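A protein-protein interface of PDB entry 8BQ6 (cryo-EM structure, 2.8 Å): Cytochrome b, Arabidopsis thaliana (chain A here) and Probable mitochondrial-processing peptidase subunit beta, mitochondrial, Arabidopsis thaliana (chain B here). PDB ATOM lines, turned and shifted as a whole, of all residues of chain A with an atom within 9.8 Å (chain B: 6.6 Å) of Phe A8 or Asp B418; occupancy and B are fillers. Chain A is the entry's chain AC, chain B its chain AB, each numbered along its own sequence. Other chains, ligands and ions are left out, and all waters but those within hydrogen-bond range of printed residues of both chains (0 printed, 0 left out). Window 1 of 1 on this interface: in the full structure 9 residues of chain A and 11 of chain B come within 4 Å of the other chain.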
ATOM      1  N   THR A   2      12.981 -16.071 -10.145  1.00  0.00           N
ATOM      2  CA  THR A   2      13.228 -14.905  -9.311  1.00  0.00           C
ATOM      3  C   THR A   2      13.589 -15.330  -7.902  1.00  0.00           C
ATOM      4  O   THR A   2      13.115 -16.351  -7.410  1.00  0.00           O
ATOM      5  CB  THR A   2      12.004 -13.985  -9.223  1.00  0.00           C
ATOM      6  OG1 THR A   2      11.121 -14.473  -8.209  1.00  0.00           O
ATOM      7  CG2 THR A   2      11.261 -13.967 -10.536  1.00  0.00           C
ATOM      8  N   ILE A   3      14.417 -14.529  -7.247  1.00  0.00           N
ATOM      9  CA  ILE A   3      14.755 -14.719  -5.844  1.00  0.00           C
ATOM     10  C   ILE A   3      13.991 -13.671  -5.052  1.00  0.00           C
ATOM     11  O   ILE A   3      14.135 -12.468  -5.300  1.00  0.00           O
ATOM     12  CB  ILE A   3      16.268 -14.611  -5.618  1.00  0.00           C
ATOM     13  CG1 ILE A   3      17.001 -15.427  -6.683  1.00  0.00           C
ATOM     14  CG2 ILE A   3      16.635 -15.094  -4.224  1.00  0.00           C
ATOM     15  CD1 ILE A   3      18.499 -15.402  -6.559  1.00  0.00           C
ATOM     16  N   ARG A   4      13.164 -14.121  -4.108  1.00  0.00           N
ATOM     17  CA  ARG A   4      12.225 -13.237  -3.417  1.00  0.00           C
ATOM     18  C   ARG A   4      12.903 -12.595  -2.206  1.00  0.00           C
ATOM     19  O   ARG A   4      12.556 -12.832  -1.047  1.00  0.00           O
ATOM     20  CB  ARG A   4      10.972 -14.003  -3.018  1.00  0.00           C
ATOM     21  CG  ARG A   4      10.687 -15.205  -3.896  1.00  0.00           C
ATOM     22  CD  ARG A   4       9.285 -15.739  -3.661  1.00  0.00           C
ATOM     23  NE  ARG A   4       8.254 -14.921  -4.291  1.00  0.00           N
ATOM     24  CZ  ARG A   4       8.019 -14.881  -5.596  1.00  0.00           C
ATOM     25  NH1 ARG A   4       8.734 -15.593  -6.450  1.00  0.00           N
ATOM     26  NH2 ARG A   4       7.037 -14.109  -6.055  1.00  0.00           N
ATOM     27  N   ASN A   5      13.898 -11.760  -2.505  1.00  0.00           N
ATOM     28  CA  ASN A   5      14.597 -11.034  -1.453  1.00  0.00           C
ATOM     29  C   ASN A   5      13.697  -9.989  -0.808  1.00  0.00           C
ATOM     30  O   ASN A   5      13.636  -9.886   0.422  1.00  0.00           O
ATOM     31  CB  ASN A   5      15.850 -10.373  -2.024  1.00  0.00           C
ATOM     32  CG  ASN A   5      16.847 -11.378  -2.550  1.00  0.00           C
ATOM     33  OD1 ASN A   5      16.686 -12.581  -2.369  1.00  0.00           O
ATOM     34  ND2 ASN A   5      17.871 -10.890  -3.235  1.00  0.00           N
ATOM     35  N   GLN A   6      12.994  -9.209  -1.618  1.00  0.00           N
ATOM     36  CA  GLN A   6      12.137  -8.142  -1.125  1.00  0.00           C
ATOM     37  C   GLN A   6      10.675  -8.551  -1.220  1.00  0.00           C
ATOM     38  O   GLN A   6      10.334  -9.649  -1.663  1.00  0.00           O
ATOM     39  CB  GLN A   6      12.381  -6.855  -1.910  1.00  0.00           C
ATOM     40  CG  GLN A   6      13.835  -6.578  -2.167  1.00  0.00           C
ATOM     41  CD  GLN A   6      14.108  -5.110  -2.344  1.00  0.00           C
ATOM     42  OE1 GLN A   6      14.110  -4.597  -3.461  1.00  0.00           O
ATOM     43  NE2 GLN A   6      14.331  -4.416  -1.237  1.00  0.00           N
ATOM     44  N   ARG A   7       9.819  -7.616  -0.806  1.00  0.00           N
ATOM     45  CA  ARG A   7       8.369  -7.909  -0.774  1.00  0.00           C
ATOM     46  C   ARG A   7       7.647  -7.252  -1.948  1.00  0.00           C
ATOM     47  O   ARG A   7       7.670  -6.014  -2.045  1.00  0.00           O
ATOM     48  CB  ARG A   7       7.768  -7.479   0.569  1.00  0.00           C
ATOM     49  CG  ARG A   7       8.165  -8.374   1.732  1.00  0.00           C
ATOM     50  CD  ARG A   7       7.244  -8.204   2.919  1.00  0.00           C
ATOM     51  NE  ARG A   7       7.118  -6.818   3.347  1.00  0.00           N
ATOM     52  CZ  ARG A   7       7.756  -6.277   4.377  1.00  0.00           C
ATOM     53  NH1 ARG A   7       8.585  -7.002   5.108  1.00  0.00           N
ATOM     54  NH2 ARG A   7       7.565  -5.005   4.675  1.00  0.00           N
ATOM     55  N   PHE A   8       7.060  -8.061  -2.816  1.00  0.00           N
ATOM     56  CA  PHE A   8       6.216  -7.605  -3.910  1.00  0.00           C
ATOM     57  C   PHE A   8       4.782  -7.475  -3.420  1.00  0.00           C
ATOM     58  O   PHE A   8       4.558  -7.261  -2.225  1.00  0.00           O
ATOM     59  CB  PHE A   8       6.333  -8.546  -5.103  1.00  0.00           C
ATOM     60  CG  PHE A   8       7.669  -8.481  -5.768  1.00  0.00           C
ATOM     61  CD1 PHE A   8       8.678  -9.354  -5.408  1.00  0.00           C
ATOM     62  CD2 PHE A   8       7.928  -7.522  -6.728  1.00  0.00           C
ATOM     63  CE1 PHE A   8       9.917  -9.285  -6.010  1.00  0.00           C
ATOM     64  CE2 PHE A   8       9.164  -7.450  -7.332  1.00  0.00           C
ATOM     65  CZ  PHE A   8      10.159  -8.331  -6.972  1.00  0.00           C
ATOM     66  N   SER A   9       3.828  -7.500  -4.349  1.00  0.00           N
ATOM     67  CA  SER A   9       2.403  -7.429  -4.040  1.00  0.00           C
ATOM     68  C   SER A   9       2.047  -8.185  -2.764  1.00  0.00           C
ATOM     69  O   SER A   9       2.466  -9.327  -2.561  1.00  0.00           O
ATOM     70  CB  SER A   9       1.604  -7.990  -5.219  1.00  0.00           C
ATOM     71  OG  SER A   9       0.228  -8.097  -4.906  1.00  0.00           O
ATOM     72  N   LEU A  10       1.280  -7.519  -1.897  1.00  0.00           N
ATOM     73  CA  LEU A  10       0.859  -8.112  -0.632  1.00  0.00           C
ATOM     74  C   LEU A  10       0.048  -9.380  -0.838  1.00  0.00           C
ATOM     75  O   LEU A  10      -0.001 -10.237   0.051  1.00  0.00           O
ATOM     76  CB  LEU A  10       0.034  -7.107   0.170  1.00  0.00           C
ATOM     77  CG  LEU A  10       0.782  -5.948   0.825  1.00  0.00           C
ATOM     78  CD1 LEU A  10       1.973  -6.468   1.607  1.00  0.00           C
ATOM     79  CD2 LEU A  10       1.224  -4.936  -0.218  1.00  0.00           C
ATOM     80  N   LEU A  11      -0.606  -9.510  -1.993  1.00  0.00           N
ATOM     81  CA  LEU A  11      -1.418 -10.691  -2.251  1.00  0.00           C
ATOM     82  C   LEU A  11      -0.574 -11.951  -2.330  1.00  0.00           C
ATOM     83  O   LEU A  11      -1.066 -13.047  -2.047  1.00  0.00           O
ATOM     84  CB  LEU A  11      -2.209 -10.502  -3.540  1.00  0.00           C
ATOM     85  CG  LEU A  11      -3.303  -9.446  -3.433  1.00  0.00           C
ATOM     86  CD1 LEU A  11      -4.001  -9.285  -4.765  1.00  0.00           C
ATOM     87  CD2 LEU A  11      -4.284  -9.823  -2.337  1.00  0.00           C
ATOM     88  N   LYS A  12       0.693 -11.822  -2.707  1.00  0.00           N
ATOM     89  CA  LYS A  12       1.572 -12.973  -2.826  1.00  0.00           C
ATOM     90  C   LYS A  12       2.404 -13.221  -1.577  1.00  0.00           C
ATOM     91  O   LYS A  12       3.215 -14.151  -1.568  1.00  0.00           O
ATOM     92  CB  LYS A  12       2.480 -12.814  -4.043  1.00  0.00           C
ATOM     93  CG  LYS A  12       1.732 -12.971  -5.347  1.00  0.00           C
ATOM     94  CD  LYS A  12       2.389 -12.203  -6.461  1.00  0.00           C
ATOM     95  CE  LYS A  12       2.436 -13.053  -7.711  1.00  0.00           C
ATOM     96  NZ  LYS A  12       1.156 -12.986  -8.468  1.00  0.00           N
ATOM     97  N   GLN A  13       2.228 -12.420  -0.531  1.00  0.00           N
ATOM     98  CA  GLN A  13       2.848 -12.707   0.751  1.00  0.00           C
ATOM     99  C   GLN A  13       2.204 -13.946   1.368  1.00  0.00           C
ATOM    100  O   GLN A  13       1.072 -14.299   1.031  1.00  0.00           O
ATOM    101  CB  GLN A  13       2.697 -11.513   1.689  1.00  0.00           C
ATOM    102  CG  GLN A  13       3.686 -10.395   1.438  1.00  0.00           C
ATOM    103  CD  GLN A  13       5.090 -10.903   1.196  1.00  0.00           C
ATOM    104  OE1 GLN A  13       5.700 -11.521   2.067  1.00  0.00           O
ATOM    105  NE2 GLN A  13       5.606 -10.656   0.002  1.00  0.00           N
ATOM    106  N   PRO A  14       2.906 -14.632   2.273  1.00  0.00           N
ATOM    107  CA  PRO A  14       2.300 -15.812   2.913  1.00  0.00           C
ATOM    108  C   PRO A  14       1.066 -15.491   3.740  1.00  0.00           C
ATOM    109  O   PRO A  14       0.279 -16.401   4.023  1.00  0.00           O
ATOM    110  CB  PRO A  14       3.436 -16.376   3.781  1.00  0.00           C
ATOM    111  CG  PRO A  14       4.674 -15.665   3.350  1.00  0.00           C
ATOM    112  CD  PRO A  14       4.255 -14.356   2.794  1.00  0.00           C
ATOM    113  N   ILE A  15       0.866 -14.230   4.130  1.00  0.00           N
ATOM    114  CA  ILE A  15      -0.331 -13.865   4.885  1.00  0.00           C
ATOM    115  C   ILE A  15      -1.579 -14.043   4.027  1.00  0.00           C
ATOM    116  O   ILE A  15      -2.653 -14.392   4.534  1.00  0.00           O
ATOM    117  CB  ILE A  15      -0.208 -12.426   5.424  1.00  0.00           C
ATOM    118  CG1 ILE A  15      -1.460 -12.013   6.202  1.00  0.00           C
ATOM    119  CG2 ILE A  15       0.017 -11.443   4.292  1.00  0.00           C
ATOM    120  CD1 ILE A  15      -1.704 -12.819   7.451  1.00  0.00           C
ATOM    121  N   SER A  16      -1.465 -13.810   2.720  1.00  0.00           N
ATOM    122  CA  SER A  16      -2.620 -13.837   1.835  1.00  0.00           C
ATOM    123  C   SER A  16      -2.441 -14.704   0.597  1.00  0.00           C
ATOM    124  O   SER A  16      -3.293 -14.652  -0.297  1.00  0.00           O
ATOM    125  CB  SER A  16      -2.983 -12.410   1.402  1.00  0.00           C
ATOM    126  OG  SER A  16      -1.826 -11.606   1.268  1.00  0.00           O
ATOM    127  N   ARG B 382      15.025  -2.826  -7.502  1.00  0.00           N
ATOM    128  CA  ARG B 382      14.107  -3.953  -7.364  1.00  0.00           C
ATOM    129  C   ARG B 382      14.417  -5.045  -8.379  1.00  0.00           C
ATOM    130  O   ARG B 382      14.304  -6.238  -8.080  1.00  0.00           O
ATOM    131  CB  ARG B 382      12.663  -3.476  -7.509  1.00  0.00           C
ATOM    132  CG  ARG B 382      12.047  -3.005  -6.210  1.00  0.00           C
ATOM    133  CD  ARG B 382      10.684  -2.384  -6.431  1.00  0.00           C
ATOM    134  NE  ARG B 382      10.396  -1.325  -5.470  1.00  0.00           N
ATOM    135  CZ  ARG B 382      10.120  -1.523  -4.187  1.00  0.00           C
ATOM    136  NH1 ARG B 382      10.102  -2.737  -3.660  1.00  0.00           N
ATOM    137  NH2 ARG B 382       9.856  -0.475  -3.413  1.00  0.00           N
ATOM    138  N   VAL B 383      14.791  -4.652  -9.596  1.00  0.00           N
ATOM    139  CA  VAL B 383      15.124  -5.637 -10.621  1.00  0.00           C
ATOM    140  C   VAL B 383      16.455  -6.312 -10.309  1.00  0.00           C
ATOM    141  O   VAL B 383      16.589  -7.537 -10.414  1.00  0.00           O
ATOM    142  CB  VAL B 383      15.132  -4.979 -12.012  1.00  0.00           C
ATOM    143  CG1 VAL B 383      15.594  -5.969 -13.051  1.00  0.00           C
ATOM    144  CG2 VAL B 383      13.743  -4.471 -12.350  1.00  0.00           C
ATOM    145  N   ASN B 386      16.325  -8.614  -6.896  1.00  0.00           N
ATOM    146  CA  ASN B 386      15.530  -9.833  -6.959  1.00  0.00           C
ATOM    147  C   ASN B 386      15.729 -10.633  -8.238  1.00  0.00           C
ATOM    148  O   ASN B 386      15.095 -11.680  -8.391  1.00  0.00           O
ATOM    149  CB  ASN B 386      14.049  -9.501  -6.797  1.00  0.00           C
ATOM    150  CG  ASN B 386      13.747  -8.852  -5.475  1.00  0.00           C
ATOM    151  OD1 ASN B 386      13.484  -9.529  -4.486  1.00  0.00           O
ATOM    152  ND2 ASN B 386      13.788  -7.528  -5.445  1.00  0.00           N
ATOM    153  N   ILE B 388      14.859 -10.153 -11.497  1.00  0.00           N
ATOM    154  CA  ILE B 388      13.559 -10.349 -12.122  1.00  0.00           C
ATOM    155  C   ILE B 388      13.535  -9.872 -13.575  1.00  0.00           C
ATOM    156  O   ILE B 388      12.470  -9.787 -14.170  1.00  0.00           O
ATOM    157  CB  ILE B 388      12.433  -9.691 -11.301  1.00  0.00           C
ATOM    158  CG1 ILE B 388      12.621  -8.180 -11.207  1.00  0.00           C
ATOM    159  CG2 ILE B 388      12.349 -10.299  -9.915  1.00  0.00           C
ATOM    160  CD1 ILE B 388      11.492  -7.491 -10.490  1.00  0.00           C
ATOM    161  N   ASP B 414       8.780 -16.668 -16.309  1.00  0.00           N
ATOM    162  CA  ASP B 414       8.332 -16.755 -14.926  1.00  0.00           C
ATOM    163  C   ASP B 414       8.636 -15.505 -14.112  1.00  0.00           C
ATOM    164  O   ASP B 414       8.180 -15.408 -12.969  1.00  0.00           O
ATOM    165  CB  ASP B 414       8.961 -17.972 -14.251  1.00  0.00           C
ATOM    166  CG  ASP B 414       8.411 -19.274 -14.785  1.00  0.00           C
ATOM    167  OD1 ASP B 414       9.137 -20.288 -14.746  1.00  0.00           O
ATOM    168  OD2 ASP B 414       7.253 -19.285 -15.248  1.00  0.00           O
ATOM    169  N   CYS B 415       9.389 -14.555 -14.657  1.00  0.00           N
ATOM    170  CA  CYS B 415       9.687 -13.321 -13.945  1.00  0.00           C
ATOM    171  C   CYS B 415       8.659 -12.231 -14.202  1.00  0.00           C
ATOM    172  O   CYS B 415       8.702 -11.191 -13.535  1.00  0.00           O
ATOM    173  CB  CYS B 415      11.070 -12.802 -14.348  1.00  0.00           C
ATOM    174  SG  CYS B 415      12.462 -13.769 -13.734  1.00  0.00           S
ATOM    175  N   LEU B 416       7.728 -12.462 -15.130  1.00  0.00           N
ATOM    176  CA  LEU B 416       6.957 -11.372 -15.716  1.00  0.00           C
ATOM    177  C   LEU B 416       5.987 -10.755 -14.720  1.00  0.00           C
ATOM    178  O   LEU B 416       5.807  -9.532 -14.700  1.00  0.00           O
ATOM    179  CB  LEU B 416       6.204 -11.875 -16.945  1.00  0.00           C
ATOM    180  CG  LEU B 416       7.031 -12.069 -18.213  1.00  0.00           C
ATOM    181  CD1 LEU B 416       6.120 -12.388 -19.378  1.00  0.00           C
ATOM    182  CD2 LEU B 416       7.859 -10.833 -18.503  1.00  0.00           C
ATOM    183  N   ASP B 417       5.334 -11.578 -13.903  1.00  0.00           N
ATOM    184  CA  ASP B 417       4.325 -11.043 -12.998  1.00  0.00           C
ATOM    185  C   ASP B 417       4.949 -10.104 -11.972  1.00  0.00           C
ATOM    186  O   ASP B 417       4.388  -9.049 -11.656  1.00  0.00           O
ATOM    187  CB  ASP B 417       3.572 -12.181 -12.316  1.00  0.00           C
ATOM    188  CG  ASP B 417       2.402 -11.686 -11.504  1.00  0.00           C
ATOM    189  OD1 ASP B 417       1.313 -11.482 -12.080  1.00  0.00           O
ATOM    190  OD2 ASP B 417       2.571 -11.492 -10.288  1.00  0.00           O
ATOM    191  N   ASP B 418       6.121 -10.469 -11.450  1.00  0.00           N
ATOM    192  CA  ASP B 418       6.815  -9.610 -10.494  1.00  0.00           C
ATOM    193  C   ASP B 418       7.441  -8.402 -11.173  1.00  0.00           C
ATOM    194  O   ASP B 418       7.468  -7.306 -10.600  1.00  0.00           O
ATOM    195  CB  ASP B 418       7.883 -10.407  -9.757  1.00  0.00           C
ATOM    196  CG  ASP B 418       7.472 -10.746  -8.355  1.00  0.00           C
ATOM    197  OD1 ASP B 418       6.374 -10.316  -7.950  1.00  0.00           O
ATOM    198  OD2 ASP B 418       8.238 -11.446  -7.662  1.00  0.00           O
ATOM    199  N   LEU B 419       7.989  -8.589 -12.371  1.00  0.00           N
ATOM    200  CA  LEU B 419       8.551  -7.459 -13.099  1.00  0.00           C
ATOM    201  C   LEU B 419       7.473  -6.440 -13.435  1.00  0.00           C
ATOM    202  O   LEU B 419       7.685  -5.230 -13.296  1.00  0.00           O
ATOM    203  CB  LEU B 419       9.243  -7.954 -14.365  1.00  0.00           C
ATOM    204  CG  LEU B 419       9.921  -6.909 -15.243  1.00  0.00           C
ATOM    205  CD1 LEU B 419      11.018  -6.164 -14.494  1.00  0.00           C
ATOM    206  CD2 LEU B 419      10.465  -7.593 -16.470  1.00  0.00           C
ATOM    207  N   SER B 420       6.303  -6.916 -13.864  1.00  0.00           N
ATOM    208  CA  SER B 420       5.200  -6.021 -14.194  1.00  0.00           C
ATOM    209  C   SER B 420       4.737  -5.244 -12.974  1.00  0.00           C
ATOM    210  O   SER B 420       4.433  -4.049 -13.065  1.00  0.00           O
ATOM    211  CB  SER B 420       4.043  -6.825 -14.776  1.00  0.00           C
ATOM    212  OG  SER B 420       4.512  -7.693 -15.788  1.00  0.00           O
ATOM    213  N   TYR B 421       4.651  -5.915 -11.827  1.00  0.00           N
ATOM    214  CA  TYR B 421       4.297  -5.227 -10.594  1.00  0.00           C
ATOM    215  C   TYR B 421       5.331  -4.167 -10.248  1.00  0.00           C
ATOM    216  O   TYR B 421       4.986  -3.041  -9.872  1.00  0.00           O
ATOM    217  CB  TYR B 421       4.169  -6.234  -9.454  1.00  0.00           C
ATOM    218  CG  TYR B 421       3.975  -5.564  -8.125  1.00  0.00           C
ATOM    219  CD1 TYR B 421       2.707  -5.236  -7.685  1.00  0.00           C
ATOM    220  CD2 TYR B 421       5.059  -5.235  -7.321  1.00  0.00           C
ATOM    221  CE1 TYR B 421       2.519  -4.610  -6.481  1.00  0.00           C
ATOM    222  CE2 TYR B 421       4.879  -4.604  -6.117  1.00  0.00           C
ATOM    223  CZ  TYR B 421       3.606  -4.298  -5.702  1.00  0.00           C
ATOM    224  OH  TYR B 421       3.407  -3.672  -4.499  1.00  0.00           O
ATOM    225  N   ALA B 422       6.614  -4.523 -10.359  1.00  0.00           N
ATOM    226  CA  ALA B 422       7.686  -3.601 -10.006  1.00  0.00           C
ATOM    227  C   ALA B 422       7.670  -2.368 -10.896  1.00  0.00           C
ATOM    228  O   ALA B 422       7.816  -1.240 -10.412  1.00  0.00           O
ATOM    229  CB  ALA B 422       9.035  -4.311 -10.110  1.00  0.00           C
ATOM    230  N   ILE B 423       7.485  -2.568 -12.204  1.00  0.00           N
ATOM    231  CA  ILE B 423       7.500  -1.456 -13.148  1.00  0.00           C
ATOM    232  C   ILE B 423       6.363  -0.490 -12.855  1.00  0.00           C
ATOM    233  O   ILE B 423       6.556   0.731 -12.814  1.00  0.00           O
ATOM    234  CB  ILE B 423       7.425  -1.983 -14.591  1.00  0.00           C
ATOM    235  CG1 ILE B 423       8.728  -2.684 -14.968  1.00  0.00           C
ATOM    236  CG2 ILE B 423       7.103  -0.854 -15.552  1.00  0.00           C
ATOM    237  CD1 ILE B 423       8.631  -3.487 -16.232  1.00  0.00           C
ATOM    238  N   ASP B 515       1.913 -15.293 -18.733  1.00  0.00           N
ATOM    239  CA  ASP B 515       1.921 -14.849 -17.347  1.00  0.00           C
ATOM    240  C   ASP B 515       2.080 -13.342 -17.209  1.00  0.00           C
ATOM    241  O   ASP B 515       2.134 -12.837 -16.084  1.00  0.00           O
ATOM    242  CB  ASP B 515       3.037 -15.551 -16.578  1.00  0.00           C
ATOM    243  CG  ASP B 515       2.695 -16.979 -16.230  1.00  0.00           C
ATOM    244  OD1 ASP B 515       3.619 -17.729 -15.855  1.00  0.00           O
ATOM    245  OD2 ASP B 515       1.506 -17.352 -16.319  1.00  0.00           O
ATOM    246  N   PRO B 517       0.585  -9.814 -16.934  1.00  0.00           N
ATOM    247  CA  PRO B 517      -0.764  -9.387 -16.548  1.00  0.00           C
ATOM    248  C   PRO B 517      -1.498  -8.710 -17.695  1.00  0.00           C
ATOM    249  O   PRO B 517      -0.899  -8.066 -18.558  1.00  0.00           O
ATOM    250  CB  PRO B 517      -0.512  -8.411 -15.393  1.00  0.00           C
ATOM    251  CG  PRO B 517       0.863  -8.725 -14.914  1.00  0.00           C
ATOM    252  CD  PRO B 517       1.627  -9.213 -16.090  1.00  0.00           C
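The side-chain carboxylate (OD2) of Asp B417 lies within salt-bridge range of the side-chain amino group (NZ) of Lys A12.
The side-chain amide oxygen (OD1) of Asn B386 is in hydrogen-bond range of the backbone NH (N) of Gln A6, at 2.9 Å.
The side-chain amide oxygen of Asn B386 lies within hydrogen-bond range of the backbone NH of Asn A5 (3.0 Å).
The side-chain carboxylate (OD2) of Asp B418 lies within salt-bridge range of the guanidinium group (NH2) of Arg A4 (3.3 Å).
The side-chain amide oxygen of Asn B386 sits close to the backbone carbonyl oxygen of Ile A3 (3.1 Å).
Printed residues of chain B within 4 Å of Asn A5: Asn B386.
Of the printed residues of chain B, Gln A6 touches Arg B382 and Asn B386.
Of the printed residues of chain A, Arg B382 touches Gln A6.
Asp B417 touches just one residue of chain A: Lys A12 (2.7 Å).
Of chain A, only Arg A4 (3.3 Å) and Phe A8 (3.1 Å) come within 4 Å of Asp B418.
No residue of chain A comes within 4 Å of Ser B420.
The nearest residue of chain A that does not touch Asp B418 is Thr A2 (4.2 Å).
The nearest printed residue of chain B that does not touch Ser A9 is Asp B418 (5.2 Å).
Among the printed residues, pairs that only touch across the chains: Phe A8 with Asp B418 (3.1 Å), Thr A2 with Cys B415 (3.4 Å), Ser A9 with Tyr B421 (3.5 Å), Phe A8 with Tyr B421 (3.7 Å), Thr A2 with Ile B388 (3.8 Å), Gln A6 with Arg B382 (3.8 Å), Thr A2 with Asn B386 (3.8 Å), Phe A8 with Ile B388 (3.9 Å), Arg A4 with Asn B386 (3.9 Å) and Phe A8 with Asn B386 (3.9 Å).
Of the 16 printed residues of chain B, 7 touch a printed residue of chain A.
Printed residues of chain B that touch a printed residue of chain A: Arg B382, Asn B386, Ile B388, Cys B415, Asp B417, Asp B418 and Tyr B421.
Hydrophobic or aromatic side chains of chain B that line the printed part of chain A: Ile B388 and Tyr B421.
Along chain B the printed residues that touch a printed residue of chain A span positions 382 to 421.
Hydrophobic or aromatic side chains of chain A within 4 Å of the printed part of chain B: Phe A8.
Among the printed residues, Asp or Glu carboxylates within 4 Å of a Lys or Arg side-chain nitrogen of the other chain: Arg A4 with Asp B418 and Lys A12 with Asp B417.
The side-chain hydroxyl (OG1) of Thr A2 is in hydrogen-bond range of the guanidinium group (NH1) of Arg A4, 3.2 Å away.
OG of Ser A9 sits close to N of Leu A11 (3.3 Å).
ND2 of Asn B386 is in hydrogen-bond range of O of Arg B382 (3.0 Å).
O of Val B383 sits at hydrogen-bond distance from N of Ile B388.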
